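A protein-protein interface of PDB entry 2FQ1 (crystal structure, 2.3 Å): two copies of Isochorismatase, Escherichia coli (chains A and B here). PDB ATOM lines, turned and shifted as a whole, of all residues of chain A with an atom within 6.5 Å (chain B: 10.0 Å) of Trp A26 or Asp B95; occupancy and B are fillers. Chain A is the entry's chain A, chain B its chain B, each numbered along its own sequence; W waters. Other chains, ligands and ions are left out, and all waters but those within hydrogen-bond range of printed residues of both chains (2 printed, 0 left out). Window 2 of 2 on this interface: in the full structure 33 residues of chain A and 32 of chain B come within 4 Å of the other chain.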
ATOM      1  N   LYS A  23      19.122  14.482   7.997  1.00  0.00           N
ATOM      2  CA  LYS A  23      20.069  13.678   7.207  1.00  0.00           C
ATOM      3  C   LYS A  23      21.255  13.202   8.051  1.00  0.00           C
ATOM      4  O   LYS A  23      21.613  12.000   8.031  1.00  0.00           O
ATOM      5  CB  LYS A  23      20.570  14.446   5.983  1.00  0.00           C
ATOM      6  CG  LYS A  23      20.069  13.904   4.683  1.00  0.00           C
ATOM      7  CD  LYS A  23      20.281  14.885   3.539  1.00  0.00           C
ATOM      8  CE  LYS A  23      20.061  14.200   2.194  1.00  0.00           C
ATOM      9  NZ  LYS A  23      19.425  15.145   1.227  1.00  0.00           N
ATOM     10  N   VAL A  24      21.848  14.145   8.789  1.00  0.00           N
ATOM     11  CA  VAL A  24      22.953  13.845   9.713  1.00  0.00           C
ATOM     12  C   VAL A  24      22.521  13.433  11.124  1.00  0.00           C
ATOM     13  O   VAL A  24      21.356  13.604  11.504  1.00  0.00           O
ATOM     14  CB  VAL A  24      23.999  14.975   9.767  1.00  0.00           C
ATOM     15  CG1 VAL A  24      24.647  15.124   8.424  1.00  0.00           C
ATOM     16  CG2 VAL A  24      23.368  16.298  10.220  1.00  0.00           C
ATOM     17  N   ASP A  25      23.488  12.902  11.878  1.00  0.00           N
ATOM     18  CA  ASP A  25      23.274  12.208  13.146  1.00  0.00           C
ATOM     19  C   ASP A  25      24.024  12.832  14.313  1.00  0.00           C
ATOM     20  O   ASP A  25      23.963  12.317  15.441  1.00  0.00           O
ATOM     21  CB  ASP A  25      23.773  10.763  13.026  1.00  0.00           C
ATOM     22  CG  ASP A  25      22.650   9.757  12.965  1.00  0.00           C
ATOM     23  OD1 ASP A  25      21.504  10.157  12.661  1.00  0.00           O
ATOM     24  OD2 ASP A  25      22.920   8.561  13.220  1.00  0.00           O
ATOM     25  N   TRP A  26      24.746  13.916  14.045  1.00  0.00           N
ATOM     26  CA  TRP A  26      25.720  14.432  14.999  1.00  0.00           C
ATOM     27  C   TRP A  26      25.154  14.475  16.410  1.00  0.00           C
ATOM     28  O   TRP A  26      24.095  15.052  16.644  1.00  0.00           O
ATOM     29  CB  TRP A  26      26.212  15.812  14.587  1.00  0.00           C
ATOM     30  CG  TRP A  26      26.627  15.915  13.160  1.00  0.00           C
ATOM     31  CD1 TRP A  26      27.347  15.000  12.444  1.00  0.00           C
ATOM     32  CD2 TRP A  26      26.380  17.018  12.275  1.00  0.00           C
ATOM     33  NE1 TRP A  26      27.550  15.459  11.168  1.00  0.00           N
ATOM     34  CE2 TRP A  26      26.965  16.693  11.034  1.00  0.00           C
ATOM     35  CE3 TRP A  26      25.712  18.243  12.408  1.00  0.00           C
ATOM     36  CZ2 TRP A  26      26.895  17.550   9.922  1.00  0.00           C
ATOM     37  CZ3 TRP A  26      25.658  19.099  11.310  1.00  0.00           C
ATOM     38  CH2 TRP A  26      26.247  18.744  10.080  1.00  0.00           C
ATOM     39  N   ALA A  27      25.845  13.820  17.333  1.00  0.00           N
ATOM     40  CA  ALA A  27      25.495  13.904  18.738  1.00  0.00           C
ATOM     41  C   ALA A  27      26.000  15.240  19.258  1.00  0.00           C
ATOM     42  O   ALA A  27      27.083  15.699  18.872  1.00  0.00           O
ATOM     43  CB  ALA A  27      26.112  12.727  19.535  1.00  0.00           C
ATOM     44  N   PHE A  28      25.204  15.877  20.112  1.00  0.00           N
ATOM     45  CA  PHE A  28      25.619  17.117  20.755  1.00  0.00           C
ATOM     46  C   PHE A  28      26.808  16.893  21.699  1.00  0.00           C
ATOM     47  O   PHE A  28      26.735  16.067  22.612  1.00  0.00           O
ATOM     48  CB  PHE A  28      24.449  17.737  21.513  1.00  0.00           C
ATOM     49  CG  PHE A  28      24.805  19.008  22.240  1.00  0.00           C
ATOM     50  CD1 PHE A  28      24.692  19.088  23.622  1.00  0.00           C
ATOM     51  CD2 PHE A  28      25.258  20.124  21.535  1.00  0.00           C
ATOM     52  CE1 PHE A  28      25.018  20.256  24.291  1.00  0.00           C
ATOM     53  CE2 PHE A  28      25.591  21.290  22.197  1.00  0.00           C
ATOM     54  CZ  PHE A  28      25.476  21.355  23.580  1.00  0.00           C
ATOM     55  N   GLN A 147      30.598  23.013  16.931  1.00  0.00           N
ATOM     56  CA  GLN A 147      29.141  22.926  16.960  1.00  0.00           C
ATOM     57  C   GLN A 147      28.573  24.276  17.401  1.00  0.00           C
ATOM     58  O   GLN A 147      29.036  24.846  18.379  1.00  0.00           O
ATOM     59  CB  GLN A 147      28.691  21.820  17.919  1.00  0.00           C
ATOM     60  CG  GLN A 147      29.288  20.457  17.600  1.00  0.00           C
ATOM     61  CD  GLN A 147      28.641  19.309  18.360  1.00  0.00           C
ATOM     62  OE1 GLN A 147      27.975  19.500  19.387  1.00  0.00           O
ATOM     63  NE2 GLN A 147      28.825  18.101  17.845  1.00  0.00           N
ATOM     64  N   PHE A 167      27.951  25.324   8.525  1.00  0.00           N
ATOM     65  CA  PHE A 167      28.110  24.118   7.709  1.00  0.00           C
ATOM     66  C   PHE A 167      29.237  24.201   6.674  1.00  0.00           C
ATOM     67  O   PHE A 167      30.094  23.288   6.602  1.00  0.00           O
ATOM     68  CB  PHE A 167      26.763  23.792   7.038  1.00  0.00           C
ATOM     69  CG  PHE A 167      26.774  22.578   6.136  1.00  0.00           C
ATOM     70  CD1 PHE A 167      26.886  21.275   6.664  1.00  0.00           C
ATOM     71  CD2 PHE A 167      26.607  22.722   4.770  1.00  0.00           C
ATOM     72  CE1 PHE A 167      26.871  20.142   5.827  1.00  0.00           C
ATOM     73  CE2 PHE A 167      26.601  21.592   3.916  1.00  0.00           C
ATOM     74  CZ  PHE A 167      26.733  20.302   4.446  1.00  0.00           C
ATOM     75  N   ILE A 171      31.596  23.876  10.663  1.00  0.00           N
ATOM     76  CA  ILE A 171      30.917  23.967  11.948  1.00  0.00           C
ATOM     77  C   ILE A 171      29.528  23.322  11.833  1.00  0.00           C
ATOM     78  O   ILE A 171      28.757  23.625  10.919  1.00  0.00           O
ATOM     79  CB  ILE A 171      30.828  25.454  12.420  1.00  0.00           C
ATOM     80  CG1 ILE A 171      32.241  26.034  12.605  1.00  0.00           C
ATOM     81  CG2 ILE A 171      30.018  25.607  13.716  1.00  0.00           C
ATOM     82  CD1 ILE A 171      32.294  27.556  12.418  1.00  0.00           C
ATOM     83  N   LYS A 172      29.232  22.424  12.767  1.00  0.00           N
ATOM     84  CA  LYS A 172      27.957  21.734  12.836  1.00  0.00           C
ATOM     85  C   LYS A 172      26.869  22.601  13.500  1.00  0.00           C
ATOM     86  O   LYS A 172      26.889  22.803  14.720  1.00  0.00           O
ATOM     87  CB  LYS A 172      28.123  20.422  13.596  1.00  0.00           C
ATOM     88  CG  LYS A 172      29.182  19.483  13.024  1.00  0.00           C
ATOM     89  CD  LYS A 172      29.405  18.287  13.935  1.00  0.00           C
ATOM     90  CE  LYS A 172      30.522  17.403  13.391  1.00  0.00           C
ATOM     91  NZ  LYS A 172      30.871  16.331  14.328  1.00  0.00           N
ATOM     92  N   PRO A 173      25.911  23.116  12.695  1.00  0.00           N
ATOM     93  CA  PRO A 173      24.765  23.841  13.238  1.00  0.00           C
ATOM     94  C   PRO A 173      23.743  22.954  13.954  1.00  0.00           C
ATOM     95  O   PRO A 173      23.471  21.836  13.512  1.00  0.00           O
ATOM     96  CB  PRO A 173      24.141  24.498  11.998  1.00  0.00           C
ATOM     97  CG  PRO A 173      24.559  23.676  10.878  1.00  0.00           C
ATOM     98  CD  PRO A 173      25.868  23.054  11.219  1.00  0.00           C
ATOM     99  N   PHE A 174      23.221  23.453  15.076  1.00  0.00           N
ATOM    100  CA  PHE A 174      22.082  22.851  15.760  1.00  0.00           C
ATOM    101  C   PHE A 174      20.990  23.915  15.846  1.00  0.00           C
ATOM    102  O   PHE A 174      21.027  24.760  16.741  1.00  0.00           O
ATOM    103  CB  PHE A 174      22.481  22.335  17.156  1.00  0.00           C
ATOM    104  CG  PHE A 174      23.297  21.037  17.133  1.00  0.00           C
ATOM    105  CD1 PHE A 174      24.640  21.028  16.725  1.00  0.00           C
ATOM    106  CD2 PHE A 174      22.730  19.835  17.551  1.00  0.00           C
ATOM    107  CE1 PHE A 174      25.391  19.829  16.712  1.00  0.00           C
ATOM    108  CE2 PHE A 174      23.468  18.642  17.548  1.00  0.00           C
ATOM    109  CZ  PHE A 174      24.796  18.641  17.117  1.00  0.00           C
ATOM    110  N   SER A 199      22.018  21.185   5.791  1.00  0.00           N
ATOM    111  CA  SER A 199      23.094  21.867   6.525  1.00  0.00           C
ATOM    112  C   SER A 199      23.321  21.503   8.001  1.00  0.00           C
ATOM    113  O   SER A 199      24.346  21.874   8.565  1.00  0.00           O
ATOM    114  CB  SER A 199      22.931  23.375   6.396  1.00  0.00           C
ATOM    115  OG  SER A 199      21.932  23.797   7.276  1.00  0.00           O
ATOM    116  N   GLY A 200      22.393  20.801   8.642  1.00  0.00           N
ATOM    117  CA  GLY A 200      22.689  20.299   9.983  1.00  0.00           C
ATOM    118  C   GLY A 200      21.571  19.689  10.795  1.00  0.00           C
ATOM    119  O   GLY A 200      20.584  19.212  10.248  1.00  0.00           O
ATOM    120  N   ARG A 201      21.752  19.700  12.116  1.00  0.00           N
ATOM    121  CA  ARG A 201      20.790  19.123  13.039  1.00  0.00           C
ATOM    122  C   ARG A 201      19.748  20.157  13.393  1.00  0.00           C
ATOM    123  O   ARG A 201      20.071  21.334  13.541  1.00  0.00           O
ATOM    124  CB  ARG A 201      21.464  18.643  14.333  1.00  0.00           C
ATOM    125  CG  ARG A 201      22.495  17.539  14.183  1.00  0.00           C
ATOM    126  CD  ARG A 201      21.874  16.137  14.046  1.00  0.00           C
ATOM    127  NE  ARG A 201      20.567  15.977  14.697  1.00  0.00           N
ATOM    128  CZ  ARG A 201      20.375  15.531  15.939  1.00  0.00           C
ATOM    129  NH1 ARG A 201      21.399  15.197  16.712  1.00  0.00           N
ATOM    130  NH2 ARG A 201      19.143  15.425  16.422  1.00  0.00           N
ATOM    131  N   GLN B  85      38.559  14.804  -3.675  1.00  0.00           N
ATOM    132  CA  GLN B  85      38.072  15.471  -2.447  1.00  0.00           C
ATOM    133  C   GLN B  85      38.380  14.695  -1.162  1.00  0.00           C
ATOM    134  O   GLN B  85      37.619  13.792  -0.767  1.00  0.00           O
ATOM    135  CB  GLN B  85      36.563  15.776  -2.518  1.00  0.00           C
ATOM    136  CG  GLN B  85      36.142  16.841  -3.539  1.00  0.00           C
ATOM    137  CD  GLN B  85      34.674  17.258  -3.402  1.00  0.00           C
ATOM    138  OE1 GLN B  85      34.087  17.196  -2.315  1.00  0.00           O
ATOM    139  NE2 GLN B  85      34.083  17.706  -4.507  1.00  0.00           N
ATOM    140  N   SER B  86      39.473  15.066  -0.493  1.00  0.00           N
ATOM    141  CA  SER B  86      39.871  14.405   0.762  1.00  0.00           C
ATOM    142  C   SER B  86      38.769  14.560   1.806  1.00  0.00           C
ATOM    143  O   SER B  86      37.860  15.369   1.623  1.00  0.00           O
ATOM    144  CB  SER B  86      41.208  14.945   1.297  1.00  0.00           C
ATOM    145  OG  SER B  86      41.071  16.251   1.818  1.00  0.00           O
ATOM    146  N   ASP B  87      38.838  13.772   2.877  1.00  0.00           N
ATOM    147  CA  ASP B  87      37.848  13.859   3.952  1.00  0.00           C
ATOM    148  C   ASP B  87      37.921  15.196   4.699  1.00  0.00           C
ATOM    149  O   ASP B  87      36.891  15.715   5.149  1.00  0.00           O
ATOM    150  CB  ASP B  87      37.976  12.678   4.911  1.00  0.00           C
ATOM    151  CG  ASP B  87      37.709  11.348   4.227  1.00  0.00           C
ATOM    152  OD1 ASP B  87      36.598  11.147   3.692  1.00  0.00           O
ATOM    153  OD2 ASP B  87      38.621  10.498   4.219  1.00  0.00           O
ATOM    154  N   GLU B  88      39.137  15.739   4.800  1.00  0.00           N
ATOM    155  CA  GLU B  88      39.392  17.046   5.392  1.00  0.00           C
ATOM    156  C   GLU B  88      38.760  18.180   4.579  1.00  0.00           C
ATOM    157  O   GLU B  88      38.081  19.035   5.154  1.00  0.00           O
ATOM    158  CB  GLU B  88      40.898  17.283   5.553  1.00  0.00           C
ATOM    159  CG  GLU B  88      41.245  18.576   6.286  1.00  0.00           C
ATOM    160  CD  GLU B  88      42.730  18.888   6.275  1.00  0.00           C
ATOM    161  OE1 GLU B  88      43.095  20.026   5.908  1.00  0.00           O
ATOM    162  OE2 GLU B  88      43.535  17.999   6.631  1.00  0.00           O
ATOM    163  N   ARG B  90      36.435  17.841   1.950  1.00  0.00           N
ATOM    164  CA  ARG B  90      35.011  17.587   1.739  1.00  0.00           C
ATOM    165  C   ARG B  90      34.225  17.796   3.028  1.00  0.00           C
ATOM    166  O   ARG B  90      33.097  18.277   2.994  1.00  0.00           O
ATOM    167  CB  ARG B  90      34.776  16.177   1.186  1.00  0.00           C
ATOM    168  CG  ARG B  90      33.354  15.966   0.699  1.00  0.00           C
ATOM    169  CD  ARG B  90      33.220  14.872  -0.359  1.00  0.00           C
ATOM    170  NE  ARG B  90      31.807  14.546  -0.568  1.00  0.00           N
ATOM    171  CZ  ARG B  90      30.958  15.257  -1.312  1.00  0.00           C
ATOM    172  NH1 ARG B  90      31.362  16.352  -1.955  1.00  0.00           N
ATOM    173  NH2 ARG B  90      29.692  14.871  -1.412  1.00  0.00           N
ATOM    174  N   ALA B  91      34.828  17.416   4.154  1.00  0.00           N
ATOM    175  CA  ALA B  91      34.288  17.678   5.492  1.00  0.00           C
ATOM    176  C   ALA B  91      32.836  17.192   5.680  1.00  0.00           C
ATOM    177  O   ALA B  91      32.536  16.008   5.466  1.00  0.00           O
ATOM    178  CB  ALA B  91      34.440  19.168   5.852  1.00  0.00           C
ATOM    179  N   LEU B  92      31.941  18.105   6.053  1.00  0.00           N
ATOM    180  CA  LEU B  92      30.583  17.731   6.447  1.00  0.00           C
ATOM    181  C   LEU B  92      29.656  17.364   5.287  1.00  0.00           C
ATOM    182  O   LEU B  92      28.599  16.770   5.512  1.00  0.00           O
ATOM    183  CB  LEU B  92      29.951  18.825   7.302  1.00  0.00           C
ATOM    184  CG  LEU B  92      30.691  19.272   8.563  1.00  0.00           C
ATOM    185  CD1 LEU B  92      29.921  20.430   9.167  1.00  0.00           C
ATOM    186  CD2 LEU B  92      30.849  18.125   9.548  1.00  0.00           C
ATOM    187  N   LEU B  93      30.045  17.712   4.062  1.00  0.00           N
ATOM    188  CA  LEU B  93      29.324  17.261   2.861  1.00  0.00           C
ATOM    189  C   LEU B  93      29.270  15.735   2.729  1.00  0.00           C
ATOM    190  O   LEU B  93      28.331  15.218   2.139  1.00  0.00           O
ATOM    191  CB  LEU B  93      29.935  17.858   1.594  1.00  0.00           C
ATOM    192  CG  LEU B  93      29.841  19.353   1.293  1.00  0.00           C
ATOM    193  CD1 LEU B  93      30.889  19.694   0.255  1.00  0.00           C
ATOM    194  CD2 LEU B  93      28.440  19.766   0.798  1.00  0.00           C
ATOM    195  N   ASN B  94      30.277  15.033   3.265  1.00  0.00           N
ATOM    196  CA  ASN B  94      30.280  13.568   3.350  1.00  0.00           C
ATOM    197  C   ASN B  94      29.164  13.060   4.245  1.00  0.00           C
ATOM    198  O   ASN B  94      28.494  12.071   3.928  1.00  0.00           O
ATOM    199  CB  ASN B  94      31.606  13.042   3.914  1.00  0.00           C
ATOM    200  CG  ASN B  94      32.674  12.885   2.861  1.00  0.00           C
ATOM    201  OD1 ASN B  94      32.409  12.448   1.743  1.00  0.00           O
ATOM    202  ND2 ASN B  94      33.900  13.241   3.217  1.00  0.00           N
ATOM    203  N   ASP B  95      29.007  13.720   5.385  1.00  0.00           N
ATOM    204  CA  ASP B  95      27.929  13.430   6.312  1.00  0.00           C
ATOM    205  C   ASP B  95      26.568  13.703   5.638  1.00  0.00           C
ATOM    206  O   ASP B  95      25.645  12.891   5.727  1.00  0.00           O
ATOM    207  CB  ASP B  95      28.075  14.289   7.580  1.00  0.00           C
ATOM    208  CG  ASP B  95      29.353  14.005   8.361  1.00  0.00           C
ATOM    209  OD1 ASP B  95      29.350  14.231   9.585  1.00  0.00           O
ATOM    210  OD2 ASP B  95      30.363  13.558   7.787  1.00  0.00           O
ATOM    211  N   MET B  96      26.463  14.844   4.959  1.00  0.00           N
ATOM    212  CA  MET B  96      25.205  15.286   4.334  1.00  0.00           C
ATOM    213  C   MET B  96      24.815  14.493   3.062  1.00  0.00           C
ATOM    214  O   MET B  96      23.654  14.100   2.911  1.00  0.00           O
ATOM    215  CB  MET B  96      25.275  16.787   4.045  1.00  0.00           C
ATOM    216  CG  MET B  96      23.926  17.524   3.847  1.00  0.00           C
ATOM    217  SD  MET B  96      22.782  17.432   5.260  1.00  0.00           S
ATOM    218  CE  MET B  96      23.704  18.261   6.553  1.00  0.00           C
ATOM    219  N   TRP B  97      25.783  14.253   2.171  1.00  0.00           N
ATOM    220  CA  TRP B  97      25.504  13.720   0.825  1.00  0.00           C
ATOM    221  C   TRP B  97      26.169  12.383   0.483  1.00  0.00           C
ATOM    222  O   TRP B  97      25.882  11.795  -0.556  1.00  0.00           O
ATOM    223  CB  TRP B  97      25.854  14.771  -0.251  1.00  0.00           C
ATOM    224  CG  TRP B  97      25.088  16.052  -0.053  1.00  0.00           C
ATOM    225  CD1 TRP B  97      25.546  17.219   0.511  1.00  0.00           C
ATOM    226  CD2 TRP B  97      23.712  16.273  -0.366  1.00  0.00           C
ATOM    227  NE1 TRP B  97      24.543  18.156   0.548  1.00  0.00           N
ATOM    228  CE2 TRP B  97      23.405  17.604   0.013  1.00  0.00           C
ATOM    229  CE3 TRP B  97      22.710  15.483  -0.951  1.00  0.00           C
ATOM    230  CZ2 TRP B  97      22.129  18.156  -0.163  1.00  0.00           C
ATOM    231  CZ3 TRP B  97      21.445  16.033  -1.119  1.00  0.00           C
ATOM    232  CH2 TRP B  97      21.169  17.362  -0.729  1.00  0.00           C
ATOM    233  N   GLY B  98      27.033  11.898   1.365  1.00  0.00           N
ATOM    234  CA  GLY B  98      27.934  10.800   1.032  1.00  0.00           C
ATOM    235  C   GLY B  98      28.997  11.254   0.034  1.00  0.00           C
ATOM    236  O   GLY B  98      29.363  12.443  -0.001  1.00  0.00           O
ATOM    237  N   PRO B  99      29.505  10.315  -0.795  1.00  0.00           N
ATOM    238  CA  PRO B  99      30.609  10.663  -1.695  1.00  0.00           C
ATOM    239  C   PRO B  99      30.310  11.714  -2.784  1.00  0.00           C
ATOM    240  O   PRO B  99      31.230  12.369  -3.273  1.00  0.00           O
ATOM    241  CB  PRO B  99      31.017   9.312  -2.302  1.00  0.00           C
ATOM    242  CG  PRO B  99      29.849   8.414  -2.105  1.00  0.00           C
ATOM    243  CD  PRO B  99      29.111   8.896  -0.899  1.00  0.00           C
ATOM    244  N   GLY B 100      29.046  11.890  -3.155  1.00  0.00           N
ATOM    245  CA  GLY B 100      28.707  12.869  -4.194  1.00  0.00           C
ATOM    246  C   GLY B 100      29.348  12.439  -5.500  1.00  0.00           C
ATOM    247  O   GLY B 100      29.446  11.239  -5.775  1.00  0.00           O
ATOM    248  N   TYR B 128      28.437  25.134  -1.226  1.00  0.00           N
ATOM    249  CA  TYR B 128      27.193  25.554  -1.890  1.00  0.00           C
ATOM    250  C   TYR B 128      27.373  26.875  -2.599  1.00  0.00           C
ATOM    251  O   TYR B 128      27.004  27.026  -3.758  1.00  0.00           O
ATOM    252  CB  TYR B 128      26.006  25.675  -0.914  1.00  0.00           C
ATOM    253  CG  TYR B 128      25.539  24.388  -0.281  1.00  0.00           C
ATOM    254  CD1 TYR B 128      25.710  23.157  -0.920  1.00  0.00           C
ATOM    255  CD2 TYR B 128      24.869  24.406   0.948  1.00  0.00           C
ATOM    256  CE1 TYR B 128      25.273  21.973  -0.330  1.00  0.00           C
ATOM    257  CE2 TYR B 128      24.398  23.224   1.534  1.00  0.00           C
ATOM    258  CZ  TYR B 128      24.619  22.009   0.901  1.00  0.00           C
ATOM    259  OH  TYR B 128      24.161  20.826   1.491  1.00  0.00           O
HETATM  260  O   HOH W   1      31.910  21.389   6.182  1.00  0.00           O
HETATM  261  O   HOH W   2      20.991  16.840   8.438  1.00  0.00           O
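Of chain B, only Asp B95 (3.6 Å) and Met B96 (3.8 Å) come within 4 Å of Val A24.
Printed residues of chain B within 4 Å of Trp A26: Asp B95 (2.7 Å).
Printed residues of chain B within 4 Å of Phe A167: Leu B92, Met B96 and Tyr B128.
Of the printed residues of chain B, Ile A171 touches Leu B92.
No residue of chain B comes within 4 Å of Pro A173.
Ala B91 touches none of the printed residues of chain A.
Printed residues of chain A within 4 Å of Leu B92: Phe A167, Ile A171 and Lys A172.
Printed residues of chain A within 4 Å of Asp B95: Val A24 and Trp A26.
Gly B98 touches none of the printed residues of chain A.
Printed residues of chain A within 4 Å of Tyr B128: Phe A167 (3.5 Å).
The nearest residue of chain A that does not touch Asp B95 is Lys A23 (4.7 Å).
The backbone carbonyl oxygen of Trp A26 lies within hydrogen-bond range of the guanidinium group of Arg A201 (2.7 Å).
NE1 of Trp B97 is in hydrogen-bond range of OH of Tyr B128 (2.9 Å).
No position is printed for both chains.
Of the 12 pairs that touch across the chains among the printed residues, none has its exchanged pair printed and touching as well.
Among the printed residues, pairs that only touch across the chains: Lys A23 with Met B96 (3.5 Å), Lys A23 with Trp B97 (3.2 Å), Val A24 with Asp B95 (3.6 Å), Val A24 with Met B96 (3.8 Å), Phe A167 with Leu B92 (3.7 Å), Phe A167 with Met B96 (3.8 Å), Phe A167 with Tyr B128 (3.5 Å), Ile A171 with Leu B92 (3.8 Å), Lys A172 with Leu B92 (3.9 Å), Ser A199 with Met B96 (3.5 Å) and Gly A200 with Met B96 (3.5 Å).
Water W1 lies within hydrogen-bond range of O of Phe A167 (2.7 Å) and N of Leu B92 (3.3 Å).
Water W2 lies within hydrogen-bond range of the backbone NH of Val A24 (2.8 Å), the backbone carbonyl oxygen of Gly A200 (3.0 Å), the backbone NH of Lys A23 (3.0 Å) and the side-chain sulfur of Met B96 (3.7 Å).
Hydrophobic or aromatic side chains of chain A within 4 Å of the printed part of chain B: Val A24, Trp A26 and Phe A167.
Of the 16 printed residues of chain B, 5 touch a printed residue of chain A.
Hydrophobic or aromatic side chains of chain B within 4 Å of the printed part of chain A: Leu B92, Met B96, Trp B97 and Tyr B128.
Among the printed residues, 12 pairs touch across the chains.
The side-chain carboxylate of Asp B95 is in hydrogen-bond range of the indole nitrogen of Trp A26 (2.7 Å).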
